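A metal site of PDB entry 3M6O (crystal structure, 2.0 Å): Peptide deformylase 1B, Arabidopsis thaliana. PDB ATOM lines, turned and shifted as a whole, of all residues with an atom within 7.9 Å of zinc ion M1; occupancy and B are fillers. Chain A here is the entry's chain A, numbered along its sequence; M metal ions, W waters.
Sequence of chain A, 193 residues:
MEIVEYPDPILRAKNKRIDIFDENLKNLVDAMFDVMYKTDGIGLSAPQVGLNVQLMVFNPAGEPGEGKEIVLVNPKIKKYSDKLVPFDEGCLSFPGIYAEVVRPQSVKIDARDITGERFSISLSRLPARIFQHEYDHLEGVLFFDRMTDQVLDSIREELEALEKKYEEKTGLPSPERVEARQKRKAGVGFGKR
A ring nitrogen (NE2) of His 137 sits close to the side-chain amide nitrogen of Gln 48 (3.2 Å). The side-chain amide nitrogen of Gln 48 sits close to the side-chain sulfur of Cys 91. SG of Cys 91 sits close to N of Ser 93 (3.7 Å). ND1 of His 133 is in hydrogen-bond range of OE1 of Glu 89 (2.5 Å). The side-chain hydroxyl of Ser 93 is in hydrogen-bond range of the side-chain amide nitrogen of Gln 48 (2.9 Å). The backbone carbonyl oxygen of Gln 48 lies within hydrogen-bond range of the backbone NH of Val 4 (2.8 Å). N of Ser 45 is in hydrogen-bond range of OE2 of Glu 134, 3.1 Å away.
Zinc ion M1 is bound by water W1 (2.0 Å), NE2 of His 137 (2.1 Å), SG of Cys 91 (2.1 Å) and NE2 of His 133 (2.2 Å).
Gln 48 touches zinc ion M1. Glu 134 touches zinc ion M1 (OE1 to ZN, 3.8 Å). Within 4 Å of zinc ion M1: Gln 48, Cys 91, His 133, Glu 134 and His 137.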
ATOM      1  N   ILE A   3     -17.090  -0.560  -3.698  1.00  0.00           N
ATOM      2  CA  ILE A   3     -17.604   0.383  -4.721  1.00  0.00           C
ATOM      3  C   ILE A   3     -17.029   1.748  -4.439  1.00  0.00           C
ATOM      4  O   ILE A   3     -17.138   2.260  -3.321  1.00  0.00           O
ATOM      5  CB  ILE A   3     -19.177   0.399  -4.888  1.00  0.00           C
ATOM      6  CG1 ILE A   3     -19.611  -0.907  -5.504  1.00  0.00           C
ATOM      7  CG2 ILE A   3     -19.722   1.539  -5.868  1.00  0.00           C
ATOM      8  CD1 ILE A   3     -20.204  -1.841  -4.450  1.00  0.00           C
ATOM      9  N   VAL A   4     -16.400   2.308  -5.470  1.00  0.00           N
ATOM     10  CA  VAL A   4     -15.860   3.666  -5.492  1.00  0.00           C
ATOM     11  C   VAL A   4     -16.969   4.659  -5.674  1.00  0.00           C
ATOM     12  O   VAL A   4     -17.819   4.527  -6.591  1.00  0.00           O
ATOM     13  CB  VAL A   4     -14.821   3.860  -6.635  1.00  0.00           C
ATOM     14  CG1 VAL A   4     -14.247   5.268  -6.672  1.00  0.00           C
ATOM     15  CG2 VAL A   4     -13.742   2.832  -6.541  1.00  0.00           C
ATOM     16  N   LEU A  11     -12.959   7.490 -10.771  1.00  0.00           N
ATOM     17  CA  LEU A  11     -14.189   7.514 -11.597  1.00  0.00           C
ATOM     18  C   LEU A  11     -14.106   8.521 -12.718  1.00  0.00           C
ATOM     19  O   LEU A  11     -15.064   8.650 -13.523  1.00  0.00           O
ATOM     20  CB  LEU A  11     -15.433   7.856 -10.759  1.00  0.00           C
ATOM     21  CG  LEU A  11     -15.952   6.777  -9.794  1.00  0.00           C
ATOM     22  CD1 LEU A  11     -17.003   7.380  -8.920  1.00  0.00           C
ATOM     23  CD2 LEU A  11     -16.432   5.594 -10.600  1.00  0.00           C
ATOM     24  N   GLY A  43     -25.338  -4.397 -14.767  1.00  0.00           N
ATOM     25  CA  GLY A  43     -23.948  -4.151 -15.302  1.00  0.00           C
ATOM     26  C   GLY A  43     -23.031  -3.561 -14.241  1.00  0.00           C
ATOM     27  O   GLY A  43     -23.527  -2.885 -13.348  1.00  0.00           O
ATOM     28  N   LEU A  44     -21.713  -3.839 -14.316  1.00  0.00           N
ATOM     29  CA  LEU A  44     -20.658  -3.258 -13.459  1.00  0.00           C
ATOM     30  C   LEU A  44     -19.382  -3.064 -14.245  1.00  0.00           C
ATOM     31  O   LEU A  44     -18.893  -4.014 -14.900  1.00  0.00           O
ATOM     32  CB  LEU A  44     -20.391  -4.117 -12.228  1.00  0.00           C
ATOM     33  CG  LEU A  44     -19.339  -3.670 -11.201  1.00  0.00           C
ATOM     34  CD1 LEU A  44     -19.618  -2.337 -10.516  1.00  0.00           C
ATOM     35  CD2 LEU A  44     -19.296  -4.707 -10.171  1.00  0.00           C
ATOM     36  N   SER A  45     -18.845  -1.835 -14.219  1.00  0.00           N
ATOM     37  CA  SER A  45     -17.607  -1.476 -14.939  1.00  0.00           C
ATOM     38  C   SER A  45     -16.473  -1.450 -13.933  1.00  0.00           C
ATOM     39  O   SER A  45     -16.696  -1.131 -12.785  1.00  0.00           O
ATOM     40  CB  SER A  45     -17.754  -0.114 -15.544  1.00  0.00           C
ATOM     41  OG  SER A  45     -18.127   0.766 -14.439  1.00  0.00           O
ATOM     42  N   GLN A  48     -15.611   1.410 -11.279  1.00  0.00           N
ATOM     43  CA  GLN A  48     -16.447   1.388 -10.078  1.00  0.00           C
ATOM     44  C   GLN A  48     -15.930   0.450  -8.965  1.00  0.00           C
ATOM     45  O   GLN A  48     -16.174   0.694  -7.788  1.00  0.00           O
ATOM     46  CB  GLN A  48     -17.881   1.088 -10.498  1.00  0.00           C
ATOM     47  CG  GLN A  48     -18.606   2.346 -10.938  1.00  0.00           C
ATOM     48  CD  GLN A  48     -20.071   2.086 -11.062  1.00  0.00           C
ATOM     49  OE1 GLN A  48     -20.459   1.219 -11.825  1.00  0.00           O
ATOM     50  NE2 GLN A  48     -20.917   2.857 -10.321  1.00  0.00           N
ATOM     51  N   GLU A  89     -32.473   7.269 -13.224  1.00  0.00           N
ATOM     52  CA  GLU A  89     -31.222   6.573 -13.145  1.00  0.00           C
ATOM     53  C   GLU A  89     -30.733   6.647 -11.725  1.00  0.00           C
ATOM     54  O   GLU A  89     -31.019   7.618 -11.021  1.00  0.00           O
ATOM     55  CB  GLU A  89     -30.193   7.148 -14.117  1.00  0.00           C
ATOM     56  CG  GLU A  89     -30.099   6.206 -15.289  1.00  0.00           C
ATOM     57  CD  GLU A  89     -29.074   6.602 -16.318  1.00  0.00           C
ATOM     58  OE1 GLU A  89     -27.850   6.622 -16.003  1.00  0.00           O
ATOM     59  OE2 GLU A  89     -29.518   6.852 -17.466  1.00  0.00           O
ATOM     60  N   GLY A  90     -30.051   5.578 -11.303  1.00  0.00           N
ATOM     61  CA  GLY A  90     -29.309   5.580 -10.061  1.00  0.00           C
ATOM     62  C   GLY A  90     -27.924   5.227 -10.435  1.00  0.00           C
ATOM     63  O   GLY A  90     -27.617   4.965 -11.596  1.00  0.00           O
ATOM     64  N   CYS A  91     -27.055   5.172  -9.432  1.00  0.00           N
ATOM     65  CA  CYS A  91     -25.693   4.906  -9.687  1.00  0.00           C
ATOM     66  C   CYS A  91     -25.106   4.566  -8.338  1.00  0.00           C
ATOM     67  O   CYS A  91     -25.234   5.356  -7.379  1.00  0.00           O
ATOM     68  CB  CYS A  91     -24.989   6.164 -10.223  1.00  0.00           C
ATOM     69  SG  CYS A  91     -23.259   5.771 -10.664  1.00  0.00           S
ATOM     70  N   LEU A  92     -24.460   3.421  -8.261  1.00  0.00           N
ATOM     71  CA  LEU A  92     -23.828   2.975  -7.026  1.00  0.00           C
ATOM     72  C   LEU A  92     -22.731   3.879  -6.432  1.00  0.00           C
ATOM     73  O   LEU A  92     -22.301   3.742  -5.239  1.00  0.00           O
ATOM     74  CB  LEU A  92     -23.256   1.556  -7.260  1.00  0.00           C
ATOM     75  CG  LEU A  92     -24.231   0.352  -7.312  1.00  0.00           C
ATOM     76  CD1 LEU A  92     -23.476  -0.882  -7.077  1.00  0.00           C
ATOM     77  CD2 LEU A  92     -25.339   0.444  -6.303  1.00  0.00           C
ATOM     78  N   SER A  93     -22.187   4.739  -7.286  1.00  0.00           N
ATOM     79  CA  SER A  93     -21.145   5.647  -6.908  1.00  0.00           C
ATOM     80  C   SER A  93     -21.734   6.853  -6.292  1.00  0.00           C
ATOM     81  O   SER A  93     -20.981   7.734  -5.885  1.00  0.00           O
ATOM     82  CB  SER A  93     -20.171   6.014  -8.027  1.00  0.00           C
ATOM     83  OG  SER A  93     -19.627   4.800  -8.593  1.00  0.00           O
ATOM     84  N   PHE A  94     -23.086   6.903  -6.209  1.00  0.00           N
ATOM     85  CA  PHE A  94     -23.793   8.119  -5.642  1.00  0.00           C
ATOM     86  C   PHE A  94     -24.860   7.583  -4.799  1.00  0.00           C
ATOM     87  O   PHE A  94     -25.982   7.520  -5.294  1.00  0.00           O
ATOM     88  CB  PHE A  94     -24.467   8.942  -6.778  1.00  0.00           C
ATOM     89  CG  PHE A  94     -23.484   9.587  -7.742  1.00  0.00           C
ATOM     90  CD1 PHE A  94     -22.909   8.840  -8.763  1.00  0.00           C
ATOM     91  CD2 PHE A  94     -23.112  10.884  -7.593  1.00  0.00           C
ATOM     92  CE1 PHE A  94     -22.053   9.393  -9.640  1.00  0.00           C
ATOM     93  CE2 PHE A  94     -22.188  11.495  -8.484  1.00  0.00           C
ATOM     94  CZ  PHE A  94     -21.639  10.717  -9.513  1.00  0.00           C
ATOM     95  N   ILE A 130     -28.889   0.502 -18.957  1.00  0.00           N
ATOM     96  CA  ILE A 130     -27.858   0.179 -18.020  1.00  0.00           C
ATOM     97  C   ILE A 130     -26.502   0.112 -18.757  1.00  0.00           C
ATOM     98  O   ILE A 130     -25.521   0.600 -18.195  1.00  0.00           O
ATOM     99  CB  ILE A 130     -28.100  -1.152 -17.299  1.00  0.00           C
ATOM    100  CG1 ILE A 130     -29.408  -1.162 -16.458  1.00  0.00           C
ATOM    101  CG2 ILE A 130     -26.914  -1.454 -16.357  1.00  0.00           C
ATOM    102  CD1 ILE A 130     -29.638   0.040 -15.490  1.00  0.00           C
ATOM    103  N   HIS A 133     -25.169   3.559 -19.209  1.00  0.00           N
ATOM    104  CA  HIS A 133     -24.699   4.027 -17.882  1.00  0.00           C
ATOM    105  C   HIS A 133     -23.280   3.554 -17.521  1.00  0.00           C
ATOM    106  O   HIS A 133     -22.440   4.354 -17.099  1.00  0.00           O
ATOM    107  CB  HIS A 133     -25.697   3.712 -16.742  1.00  0.00           C
ATOM    108  CG  HIS A 133     -25.310   4.298 -15.415  1.00  0.00           C
ATOM    109  ND1 HIS A 133     -25.962   5.380 -14.857  1.00  0.00           N
ATOM    110  CD2 HIS A 133     -24.346   3.938 -14.528  1.00  0.00           C
ATOM    111  CE1 HIS A 133     -25.427   5.650 -13.683  1.00  0.00           C
ATOM    112  NE2 HIS A 133     -24.396   4.840 -13.499  1.00  0.00           N
ATOM    113  N   GLU A 134     -23.025   2.268 -17.750  1.00  0.00           N
ATOM    114  CA  GLU A 134     -21.779   1.633 -17.326  1.00  0.00           C
ATOM    115  C   GLU A 134     -20.670   1.867 -18.359  1.00  0.00           C
ATOM    116  O   GLU A 134     -19.473   1.732 -18.075  1.00  0.00           O
ATOM    117  CB  GLU A 134     -22.002   0.128 -17.156  1.00  0.00           C
ATOM    118  CG  GLU A 134     -23.052  -0.188 -16.109  1.00  0.00           C
ATOM    119  CD  GLU A 134     -22.556   0.261 -14.718  1.00  0.00           C
ATOM    120  OE1 GLU A 134     -23.328   0.898 -13.935  1.00  0.00           O
ATOM    121  OE2 GLU A 134     -21.367  -0.045 -14.432  1.00  0.00           O
ATOM    122  N   ASP A 136     -20.386   4.657 -20.021  1.00  0.00           N
ATOM    123  CA  ASP A 136     -19.987   5.956 -19.547  1.00  0.00           C
ATOM    124  C   ASP A 136     -18.894   5.862 -18.466  1.00  0.00           C
ATOM    125  O   ASP A 136     -17.867   6.484 -18.565  1.00  0.00           O
ATOM    126  CB  ASP A 136     -21.231   6.743 -19.112  1.00  0.00           C
ATOM    127  CG  ASP A 136     -21.946   7.408 -20.290  1.00  0.00           C
ATOM    128  OD1 ASP A 136     -22.911   8.182 -20.021  1.00  0.00           O
ATOM    129  OD2 ASP A 136     -21.538   7.147 -21.476  1.00  0.00           O
ATOM    130  N   HIS A 137     -19.088   5.061 -17.429  1.00  0.00           N
ATOM    131  CA  HIS A 137     -18.004   4.814 -16.470  1.00  0.00           C
ATOM    132  C   HIS A 137     -16.656   4.474 -17.110  1.00  0.00           C
ATOM    133  O   HIS A 137     -15.622   4.974 -16.637  1.00  0.00           O
ATOM    134  CB  HIS A 137     -18.423   3.697 -15.494  1.00  0.00           C
ATOM    135  CG  HIS A 137     -19.418   4.137 -14.474  1.00  0.00           C
ATOM    136  ND1 HIS A 137     -19.148   5.165 -13.597  1.00  0.00           N
ATOM    137  CD2 HIS A 137     -20.689   3.717 -14.192  1.00  0.00           C
ATOM    138  CE1 HIS A 137     -20.185   5.325 -12.785  1.00  0.00           C
ATOM    139  NE2 HIS A 137     -21.126   4.450 -13.101  1.00  0.00           N
ATOM    140  N   VAL A 141     -17.116   9.144 -17.568  1.00  0.00           N
ATOM    141  CA  VAL A 141     -18.319   9.991 -17.594  1.00  0.00           C
ATOM    142  C   VAL A 141     -19.303   9.463 -16.555  1.00  0.00           C
ATOM    143  O   VAL A 141     -19.476   8.245 -16.492  1.00  0.00           O
ATOM    144  CB  VAL A 141     -19.008   9.916 -18.975  1.00  0.00           C
ATOM    145  CG1 VAL A 141     -20.207  10.893 -19.048  1.00  0.00           C
ATOM    146  CG2 VAL A 141     -17.995  10.191 -20.099  1.00  0.00           C
ATOM    147  N   LEU A 142     -19.842  10.368 -15.695  1.00  0.00           N
ATOM    148  CA  LEU A 142     -20.805  10.112 -14.601  1.00  0.00           C
ATOM    149  C   LEU A 142     -22.192  10.600 -14.911  1.00  0.00           C
ATOM    150  O   LEU A 142     -22.353  11.596 -15.639  1.00  0.00           O
ATOM    151  CB  LEU A 142     -20.350  10.812 -13.296  1.00  0.00           C
ATOM    152  CG  LEU A 142     -18.978  10.438 -12.769  1.00  0.00           C
ATOM    153  CD1 LEU A 142     -18.914  10.600 -11.282  1.00  0.00           C
ATOM    154  CD2 LEU A 142     -18.742   8.999 -13.069  1.00  0.00           C
ATOM    155  N   PHE A 143     -23.226   9.955 -14.355  1.00  0.00           N
ATOM    156  CA  PHE A 143     -24.601  10.222 -14.878  1.00  0.00           C
ATOM    157  C   PHE A 143     -25.032  11.647 -14.789  1.00  0.00           C
ATOM    158  O   PHE A 143     -25.850  12.138 -15.595  1.00  0.00           O
ATOM    159  CB  PHE A 143     -25.712   9.260 -14.374  1.00  0.00           C
ATOM    160  CG  PHE A 143     -26.135   9.447 -12.936  1.00  0.00           C
ATOM    161  CD1 PHE A 143     -27.393   9.053 -12.526  1.00  0.00           C
ATOM    162  CD2 PHE A 143     -25.253   9.953 -11.957  1.00  0.00           C
ATOM    163  CE1 PHE A 143     -27.795   9.184 -11.191  1.00  0.00           C
ATOM    164  CE2 PHE A 143     -25.654  10.108 -10.665  1.00  0.00           C
ATOM    165  CZ  PHE A 143     -26.903   9.690 -10.271  1.00  0.00           C
HETATM  166 ZN    ZN M   1     -22.895   4.242 -12.077  1.00  0.00          ZN
HETATM  167 ZN    ZN M   2     -22.361   0.714 -12.061  1.00  0.00          ZN
HETATM  168  O   HOH W   1     -23.031   2.325 -11.595  1.00  0.00           O
